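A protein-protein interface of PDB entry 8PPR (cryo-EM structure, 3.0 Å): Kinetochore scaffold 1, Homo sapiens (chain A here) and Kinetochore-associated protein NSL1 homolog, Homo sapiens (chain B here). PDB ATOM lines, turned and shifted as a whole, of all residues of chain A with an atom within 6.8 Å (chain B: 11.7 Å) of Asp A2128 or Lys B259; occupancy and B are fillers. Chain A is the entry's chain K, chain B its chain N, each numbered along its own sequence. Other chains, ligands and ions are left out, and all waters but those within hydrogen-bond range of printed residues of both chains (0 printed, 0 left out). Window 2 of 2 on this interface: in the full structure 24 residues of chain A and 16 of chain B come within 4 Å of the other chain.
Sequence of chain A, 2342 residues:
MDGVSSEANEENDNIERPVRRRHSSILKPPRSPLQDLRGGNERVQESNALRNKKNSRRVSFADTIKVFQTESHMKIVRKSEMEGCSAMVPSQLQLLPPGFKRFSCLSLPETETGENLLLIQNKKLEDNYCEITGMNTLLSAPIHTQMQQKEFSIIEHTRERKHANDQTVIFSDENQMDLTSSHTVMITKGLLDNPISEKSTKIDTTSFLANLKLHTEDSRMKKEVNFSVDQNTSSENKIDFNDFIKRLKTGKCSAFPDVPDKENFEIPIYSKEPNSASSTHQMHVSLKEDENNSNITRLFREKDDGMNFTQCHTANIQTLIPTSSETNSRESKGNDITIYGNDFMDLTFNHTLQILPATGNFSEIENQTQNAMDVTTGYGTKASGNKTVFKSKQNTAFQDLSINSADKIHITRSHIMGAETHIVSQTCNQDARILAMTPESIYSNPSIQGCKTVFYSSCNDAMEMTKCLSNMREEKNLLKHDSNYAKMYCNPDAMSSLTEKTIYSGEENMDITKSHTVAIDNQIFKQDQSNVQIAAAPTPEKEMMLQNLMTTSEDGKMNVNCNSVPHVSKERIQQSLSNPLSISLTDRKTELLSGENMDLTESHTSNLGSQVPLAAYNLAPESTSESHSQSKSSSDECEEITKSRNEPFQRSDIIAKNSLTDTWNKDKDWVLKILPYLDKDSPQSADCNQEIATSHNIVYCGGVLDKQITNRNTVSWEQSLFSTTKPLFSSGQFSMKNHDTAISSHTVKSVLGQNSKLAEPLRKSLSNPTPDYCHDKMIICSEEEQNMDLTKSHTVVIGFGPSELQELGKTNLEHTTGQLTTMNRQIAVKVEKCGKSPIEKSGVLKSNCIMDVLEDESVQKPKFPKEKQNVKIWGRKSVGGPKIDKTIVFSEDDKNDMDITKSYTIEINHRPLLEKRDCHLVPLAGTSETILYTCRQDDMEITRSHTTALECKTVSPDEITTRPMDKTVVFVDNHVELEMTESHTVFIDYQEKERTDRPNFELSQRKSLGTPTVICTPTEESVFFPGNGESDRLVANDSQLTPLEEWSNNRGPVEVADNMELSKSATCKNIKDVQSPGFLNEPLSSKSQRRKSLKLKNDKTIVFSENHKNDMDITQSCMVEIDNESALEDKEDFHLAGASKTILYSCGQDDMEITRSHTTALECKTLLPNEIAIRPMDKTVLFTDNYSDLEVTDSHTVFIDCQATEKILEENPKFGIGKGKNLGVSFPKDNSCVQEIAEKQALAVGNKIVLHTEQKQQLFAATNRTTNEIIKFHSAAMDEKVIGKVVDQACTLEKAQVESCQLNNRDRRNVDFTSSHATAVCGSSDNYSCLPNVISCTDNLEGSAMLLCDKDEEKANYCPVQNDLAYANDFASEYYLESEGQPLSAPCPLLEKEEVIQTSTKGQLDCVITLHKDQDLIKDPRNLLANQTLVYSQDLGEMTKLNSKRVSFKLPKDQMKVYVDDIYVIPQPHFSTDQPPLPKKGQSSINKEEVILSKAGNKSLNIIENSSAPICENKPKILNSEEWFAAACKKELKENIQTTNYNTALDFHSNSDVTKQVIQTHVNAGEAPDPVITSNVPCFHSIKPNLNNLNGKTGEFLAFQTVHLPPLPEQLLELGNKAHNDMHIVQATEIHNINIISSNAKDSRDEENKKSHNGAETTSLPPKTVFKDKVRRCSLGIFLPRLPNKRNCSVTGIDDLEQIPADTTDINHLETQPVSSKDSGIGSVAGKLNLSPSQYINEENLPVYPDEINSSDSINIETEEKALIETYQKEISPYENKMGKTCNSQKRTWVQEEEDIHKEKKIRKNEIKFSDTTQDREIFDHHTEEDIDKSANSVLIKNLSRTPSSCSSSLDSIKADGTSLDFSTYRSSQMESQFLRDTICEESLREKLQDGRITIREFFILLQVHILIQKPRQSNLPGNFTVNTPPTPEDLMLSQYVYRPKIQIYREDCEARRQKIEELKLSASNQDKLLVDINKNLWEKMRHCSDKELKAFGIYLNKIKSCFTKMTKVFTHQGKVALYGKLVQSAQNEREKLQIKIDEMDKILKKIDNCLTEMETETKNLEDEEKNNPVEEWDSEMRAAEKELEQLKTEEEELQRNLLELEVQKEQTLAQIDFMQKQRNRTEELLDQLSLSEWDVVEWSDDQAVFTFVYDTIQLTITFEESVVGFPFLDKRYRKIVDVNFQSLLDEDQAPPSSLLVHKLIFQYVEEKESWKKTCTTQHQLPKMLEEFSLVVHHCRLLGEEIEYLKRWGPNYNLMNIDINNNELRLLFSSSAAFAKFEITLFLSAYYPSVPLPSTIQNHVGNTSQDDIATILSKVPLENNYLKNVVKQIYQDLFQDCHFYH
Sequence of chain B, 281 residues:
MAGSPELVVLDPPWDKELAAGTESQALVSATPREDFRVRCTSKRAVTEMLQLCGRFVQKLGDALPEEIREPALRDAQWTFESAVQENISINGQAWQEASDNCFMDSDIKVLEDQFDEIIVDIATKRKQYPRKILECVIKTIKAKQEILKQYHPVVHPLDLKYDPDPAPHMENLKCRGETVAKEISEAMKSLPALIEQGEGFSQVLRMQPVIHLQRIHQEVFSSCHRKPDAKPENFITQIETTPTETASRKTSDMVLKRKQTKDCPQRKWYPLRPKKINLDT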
ATOM      1  N   THR A2123      -1.901   1.041   2.743  1.00  0.00           N
ATOM      2  CA  THR A2123      -0.691   1.498   3.423  1.00  0.00           C
ATOM      3  C   THR A2123       0.423   0.466   3.318  1.00  0.00           C
ATOM      4  O   THR A2123       1.583   0.812   3.058  1.00  0.00           O
ATOM      5  CB  THR A2123      -0.999   1.798   4.890  1.00  0.00           C
ATOM      6  OG1 THR A2123      -2.171   2.616   4.981  1.00  0.00           O
ATOM      7  CG2 THR A2123       0.169   2.517   5.546  1.00  0.00           C
ATOM      8  N   GLU A2124       0.087  -0.810   3.511  1.00  0.00           N
ATOM      9  CA  GLU A2124       1.094  -1.861   3.433  1.00  0.00           C
ATOM     10  C   GLU A2124       1.637  -2.001   2.016  1.00  0.00           C
ATOM     11  O   GLU A2124       2.830  -2.260   1.825  1.00  0.00           O
ATOM     12  CB  GLU A2124       0.506  -3.183   3.922  1.00  0.00           C
ATOM     13  CG  GLU A2124       1.541  -4.207   4.335  1.00  0.00           C
ATOM     14  CD  GLU A2124       0.914  -5.432   4.964  1.00  0.00           C
ATOM     15  OE1 GLU A2124      -0.332  -5.507   4.997  1.00  0.00           O
ATOM     16  OE2 GLU A2124       1.663  -6.317   5.424  1.00  0.00           O
ATOM     17  N   GLU A2125       0.774  -1.845   1.010  1.00  0.00           N
ATOM     18  CA  GLU A2125       1.245  -1.864  -0.371  1.00  0.00           C
ATOM     19  C   GLU A2125       2.184  -0.697  -0.648  1.00  0.00           C
ATOM     20  O   GLU A2125       3.210  -0.858  -1.321  1.00  0.00           O
ATOM     21  CB  GLU A2125       0.057  -1.835  -1.329  1.00  0.00           C
ATOM     22  CG  GLU A2125      -0.710  -3.141  -1.393  1.00  0.00           C
ATOM     23  CD  GLU A2125      -1.959  -3.039  -2.243  1.00  0.00           C
ATOM     24  OE1 GLU A2125      -2.169  -1.977  -2.867  1.00  0.00           O
ATOM     25  OE2 GLU A2125      -2.729  -4.020  -2.286  1.00  0.00           O
ATOM     26  N   LEU A2126       1.843   0.490  -0.140  1.00  0.00           N
ATOM     27  CA  LEU A2126       2.712   1.648  -0.316  1.00  0.00           C
ATOM     28  C   LEU A2126       4.056   1.436   0.369  1.00  0.00           C
ATOM     29  O   LEU A2126       5.091   1.912  -0.112  1.00  0.00           O
ATOM     30  CB  LEU A2126       2.020   2.902   0.214  1.00  0.00           C
ATOM     31  CG  LEU A2126       0.926   3.449  -0.703  1.00  0.00           C
ATOM     32  CD1 LEU A2126       0.159   4.567  -0.013  1.00  0.00           C
ATOM     33  CD2 LEU A2126       1.513   3.921  -2.032  1.00  0.00           C
ATOM     34  N   LEU A2127       4.055   0.746   1.510  1.00  0.00           N
ATOM     35  CA  LEU A2127       5.313   0.372   2.145  1.00  0.00           C
ATOM     36  C   LEU A2127       6.112  -0.583   1.266  1.00  0.00           C
ATOM     37  O   LEU A2127       7.304  -0.363   1.017  1.00  0.00           O
ATOM     38  CB  LEU A2127       5.041  -0.275   3.500  1.00  0.00           C
ATOM     39  CG  LEU A2127       6.200  -1.123   4.032  1.00  0.00           C
ATOM     40  CD1 LEU A2127       7.474  -0.294   4.238  1.00  0.00           C
ATOM     41  CD2 LEU A2127       5.807  -1.896   5.277  1.00  0.00           C
ATOM     42  N   ASP A2128       5.468  -1.653   0.790  1.00  0.00           N
ATOM     43  CA  ASP A2128       6.171  -2.657  -0.001  1.00  0.00           C
ATOM     44  C   ASP A2128       6.739  -2.062  -1.283  1.00  0.00           C
ATOM     45  O   ASP A2128       7.775  -2.523  -1.775  1.00  0.00           O
ATOM     46  CB  ASP A2128       5.242  -3.834  -0.315  1.00  0.00           C
ATOM     47  CG  ASP A2128       4.910  -4.660   0.917  1.00  0.00           C
ATOM     48  OD1 ASP A2128       5.590  -4.485   1.951  1.00  0.00           O
ATOM     49  OD2 ASP A2128       3.981  -5.495   0.852  1.00  0.00           O
ATOM     50  N   GLN A2129       6.080  -1.041  -1.833  1.00  0.00           N
ATOM     51  CA  GLN A2129       6.648  -0.325  -2.969  1.00  0.00           C
ATOM     52  C   GLN A2129       7.898   0.453  -2.572  1.00  0.00           C
ATOM     53  O   GLN A2129       8.850   0.538  -3.357  1.00  0.00           O
ATOM     54  CB  GLN A2129       5.605   0.622  -3.564  1.00  0.00           C
ATOM     55  CG  GLN A2129       4.505  -0.067  -4.359  1.00  0.00           C
ATOM     56  CD  GLN A2129       3.436   0.899  -4.841  1.00  0.00           C
ATOM     57  OE1 GLN A2129       3.606   2.118  -4.775  1.00  0.00           O
ATOM     58  NE2 GLN A2129       2.320   0.358  -5.314  1.00  0.00           N
ATOM     59  N   LEU A2130       7.916   1.022  -1.368  1.00  0.00           N
ATOM     60  CA  LEU A2130       8.962   1.944  -0.942  1.00  0.00           C
ATOM     61  C   LEU A2130       9.939   1.337   0.063  1.00  0.00           C
ATOM     62  O   LEU A2130      10.562   2.079   0.827  1.00  0.00           O
ATOM     63  CB  LEU A2130       8.333   3.215  -0.366  1.00  0.00           C
ATOM     64  CG  LEU A2130       7.857   4.245  -1.398  1.00  0.00           C
ATOM     65  CD1 LEU A2130       7.071   5.366  -0.739  1.00  0.00           C
ATOM     66  CD2 LEU A2130       9.031   4.807  -2.190  1.00  0.00           C
ATOM     67  N   SER A2131      10.076   0.012   0.095  1.00  0.00           N
ATOM     68  CA  SER A2131      11.029  -0.656   0.981  1.00  0.00           C
ATOM     69  C   SER A2131      12.316  -1.028   0.253  1.00  0.00           C
ATOM     70  O   SER A2131      12.929  -2.060   0.544  1.00  0.00           O
ATOM     71  CB  SER A2131      10.392  -1.892   1.609  1.00  0.00           C
ATOM     72  OG  SER A2131      11.377  -2.751   2.155  1.00  0.00           O
ATOM     73  N   LEU A2132      12.751  -0.198  -0.696  1.00  0.00           N
ATOM     74  CA  LEU A2132      13.886  -0.538  -1.547  1.00  0.00           C
ATOM     75  C   LEU A2132      15.000   0.500  -1.458  1.00  0.00           C
ATOM     76  O   LEU A2132      15.552   0.911  -2.483  1.00  0.00           O
ATOM     77  CB  LEU A2132      13.422  -0.687  -2.997  1.00  0.00           C
ATOM     78  CG  LEU A2132      12.411  -1.811  -3.230  1.00  0.00           C
ATOM     79  CD1 LEU A2132      11.707  -1.646  -4.570  1.00  0.00           C
ATOM     80  CD2 LEU A2132      13.072  -3.178  -3.121  1.00  0.00           C
ATOM     81  N   ASP A2136      18.774   0.153   6.056  1.00  0.00           N
ATOM     82  CA  ASP A2136      17.721  -0.574   6.749  1.00  0.00           C
ATOM     83  C   ASP A2136      17.610  -0.031   8.164  1.00  0.00           C
ATOM     84  O   ASP A2136      18.623   0.117   8.854  1.00  0.00           O
ATOM     85  CB  ASP A2136      18.015  -2.075   6.778  1.00  0.00           C
ATOM     86  CG  ASP A2136      18.245  -2.649   5.396  1.00  0.00           C
ATOM     87  OD1 ASP A2136      19.270  -2.301   4.773  1.00  0.00           O
ATOM     88  OD2 ASP A2136      17.402  -3.445   4.935  1.00  0.00           O
ATOM     89  N   VAL B 255       9.281  -0.103  16.731  1.00  0.00           N
ATOM     90  CA  VAL B 255      10.137  -1.127  16.141  1.00  0.00           C
ATOM     91  C   VAL B 255      10.651  -0.668  14.783  1.00  0.00           C
ATOM     92  O   VAL B 255      11.838  -0.825  14.467  1.00  0.00           O
ATOM     93  CB  VAL B 255       9.388  -2.473  16.056  1.00  0.00           C
ATOM     94  CG1 VAL B 255       9.009  -2.957  17.453  1.00  0.00           C
ATOM     95  CG2 VAL B 255       8.154  -2.382  15.158  1.00  0.00           C
ATOM     96  N   LEU B 256       9.776  -0.060  13.977  1.00  0.00           N
ATOM     97  CA  LEU B 256      10.141   0.471  12.665  1.00  0.00           C
ATOM     98  C   LEU B 256      10.803  -0.617  11.821  1.00  0.00           C
ATOM     99  O   LEU B 256      11.748  -0.370  11.070  1.00  0.00           O
ATOM    100  CB  LEU B 256      11.044   1.704  12.806  1.00  0.00           C
ATOM    101  CG  LEU B 256      11.206   2.678  11.634  1.00  0.00           C
ATOM    102  CD1 LEU B 256       9.860   3.152  11.147  1.00  0.00           C
ATOM    103  CD2 LEU B 256      12.045   3.875  12.021  1.00  0.00           C
ATOM    104  N   LYS B 257      10.296  -1.841  11.956  1.00  0.00           N
ATOM    105  CA  LYS B 257      10.868  -3.012  11.303  1.00  0.00           C
ATOM    106  C   LYS B 257      10.023  -3.373  10.090  1.00  0.00           C
ATOM    107  O   LYS B 257       8.813  -3.595  10.212  1.00  0.00           O
ATOM    108  CB  LYS B 257      10.950  -4.196  12.269  1.00  0.00           C
ATOM    109  CG  LYS B 257      11.561  -3.859  13.616  1.00  0.00           C
ATOM    110  CD  LYS B 257      11.703  -5.089  14.500  1.00  0.00           C
ATOM    111  CE  LYS B 257      12.705  -6.070  13.918  1.00  0.00           C
ATOM    112  NZ  LYS B 257      14.039  -5.432  13.733  1.00  0.00           N
ATOM    113  N   ARG B 258      10.660  -3.420   8.926  1.00  0.00           N
ATOM    114  CA  ARG B 258      10.001  -3.802   7.689  1.00  0.00           C
ATOM    115  C   ARG B 258      10.145  -5.309   7.472  1.00  0.00           C
ATOM    116  O   ARG B 258      10.601  -6.046   8.351  1.00  0.00           O
ATOM    117  CB  ARG B 258      10.561  -2.974   6.532  1.00  0.00           C
ATOM    118  CG  ARG B 258      12.028  -3.224   6.216  1.00  0.00           C
ATOM    119  CD  ARG B 258      12.490  -2.303   5.096  1.00  0.00           C
ATOM    120  NE  ARG B 258      13.891  -2.495   4.744  1.00  0.00           N
ATOM    121  CZ  ARG B 258      14.521  -1.823   3.788  1.00  0.00           C
ATOM    122  NH1 ARG B 258      13.897  -0.910   3.060  1.00  0.00           N
ATOM    123  NH2 ARG B 258      15.806  -2.072   3.558  1.00  0.00           N
ATOM    124  N   LYS B 259       9.751  -5.781   6.295  1.00  0.00           N
ATOM    125  CA  LYS B 259       9.739  -7.195   5.955  1.00  0.00           C
ATOM    126  C   LYS B 259      10.867  -7.516   4.971  1.00  0.00           C
ATOM    127  O   LYS B 259      11.706  -6.665   4.654  1.00  0.00           O
ATOM    128  CB  LYS B 259       8.350  -7.577   5.425  1.00  0.00           C
ATOM    129  CG  LYS B 259       7.926  -6.896   4.122  1.00  0.00           C
ATOM    130  CD  LYS B 259       8.323  -7.678   2.879  1.00  0.00           C
ATOM    131  CE  LYS B 259       7.786  -7.013   1.622  1.00  0.00           C
ATOM    132  NZ  LYS B 259       8.182  -7.751   0.393  1.00  0.00           N
ATOM    133  N   GLN B 260      10.888  -8.767   4.503  1.00  0.00           N
ATOM    134  CA  GLN B 260      11.880  -9.266   3.549  1.00  0.00           C
ATOM    135  C   GLN B 260      13.286  -9.232   4.160  1.00  0.00           C
ATOM    136  O   GLN B 260      14.193  -8.536   3.696  1.00  0.00           O
ATOM    137  CB  GLN B 260      11.811  -8.488   2.225  1.00  0.00           C
ATOM    138  CG  GLN B 260      12.754  -8.979   1.126  1.00  0.00           C
ATOM    139  CD  GLN B 260      12.466 -10.405   0.699  1.00  0.00           C
ATOM    140  OE1 GLN B 260      13.195 -11.330   1.054  1.00  0.00           O
ATOM    141  NE2 GLN B 260      11.398 -10.587  -0.069  1.00  0.00           N
ATOM    142  N   THR B 261      13.439  -9.984   5.246  1.00  0.00           N
ATOM    143  CA  THR B 261      14.731 -10.207   5.882  1.00  0.00           C
ATOM    144  C   THR B 261      15.091 -11.680   5.732  1.00  0.00           C
ATOM    145  O   THR B 261      14.346 -12.552   6.193  1.00  0.00           O
ATOM    146  CB  THR B 261      14.700  -9.804   7.356  1.00  0.00           C
ATOM    147  OG1 THR B 261      13.696 -10.563   8.039  1.00  0.00           O
ATOM    148  CG2 THR B 261      14.390  -8.320   7.495  1.00  0.00           C
ATOM    149  N   LYS B 262      16.226 -11.951   5.094  1.00  0.00           N
ATOM    150  CA  LYS B 262      16.624 -13.322   4.806  1.00  0.00           C
ATOM    151  C   LYS B 262      18.131 -13.375   4.610  1.00  0.00           C
ATOM    152  O   LYS B 262      18.795 -12.346   4.465  1.00  0.00           O
ATOM    153  CB  LYS B 262      15.907 -13.864   3.566  1.00  0.00           C
ATOM    154  CG  LYS B 262      16.351 -13.209   2.270  1.00  0.00           C
ATOM    155  CD  LYS B 262      15.489 -13.648   1.101  1.00  0.00           C
ATOM    156  CE  LYS B 262      16.022 -13.093  -0.209  1.00  0.00           C
ATOM    157  NZ  LYS B 262      15.991 -11.605  -0.229  1.00  0.00           N
ATOM    158  N   ASP B 263      18.658 -14.597   4.604  1.00  0.00           N
ATOM    159  CA  ASP B 263      20.085 -14.837   4.395  1.00  0.00           C
ATOM    160  C   ASP B 263      20.386 -14.677   2.910  1.00  0.00           C
ATOM    161  O   ASP B 263      20.252 -15.611   2.118  1.00  0.00           O
ATOM    162  CB  ASP B 263      20.478 -16.220   4.899  1.00  0.00           C
ATOM    163  CG  ASP B 263      21.971 -16.460   4.832  1.00  0.00           C
ATOM    164  OD1 ASP B 263      22.702 -15.896   5.672  1.00  0.00           O
ATOM    165  OD2 ASP B 263      22.416 -17.210   3.938  1.00  0.00           O
ATOM    166  N   CYS B 264      20.799 -13.472   2.530  1.00  0.00           N
ATOM    167  CA  CYS B 264      21.107 -13.185   1.142  1.00  0.00           C
ATOM    168  C   CYS B 264      22.375 -13.920   0.713  1.00  0.00           C
ATOM    169  O   CYS B 264      23.212 -14.271   1.547  1.00  0.00           O
ATOM    170  CB  CYS B 264      21.278 -11.682   0.942  1.00  0.00           C
ATOM    171  SG  CYS B 264      22.535 -10.936   2.004  1.00  0.00           S
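Of the 11 printed residues of chain A, 4 touch a printed residue of chain B. Along chain A the printed residues that touch a printed residue of chain B span positions 2128 to 2136. Among the printed residues, 4 pairs touch across the chains. Among the printed residues, Asp or Glu carboxylates within 4 Å of a Lys or Arg side-chain nitrogen of the other chain: Asp A2136 with Arg B258 (2.5 Å).
No residue of chain B comes within 4 Å of Glu A2124. Glu A2125 touches none of the printed residues of chain B. Leu A2126 touches none of the printed residues of chain B. No residue of chain B comes within 4 Å of Gln A2129. Leu A2130 touches none of the printed residues of chain B. Ser A2131 touches one residue of chain B. Of the printed residues of chain B, Leu A2132 touches Arg B258. Of the printed residues of chain B, Asp A2136 touches Arg B258. Of the printed residues of chain A, Arg B258 touches Ser A2131 (2.9 Å), Leu A2132 (3.99 Å) and Asp A2136 (2.5 Å).
The guanidinium group (NH1) of Arg B258 sits at hydrogen-bond distance from the backbone carbonyl oxygen (O) of Ser A2131 (2.9 Å). The guanidinium group (NH2) of Arg B258 is in salt-bridge range of the side-chain carboxylate (OD2) of Asp A2136 (2.5 Å).
Among the printed residues, merely in contact across the chains: Asp A2128 with Lys B259 (3.4 Å) and Leu A2132 with Arg B258 (3.99 Å).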
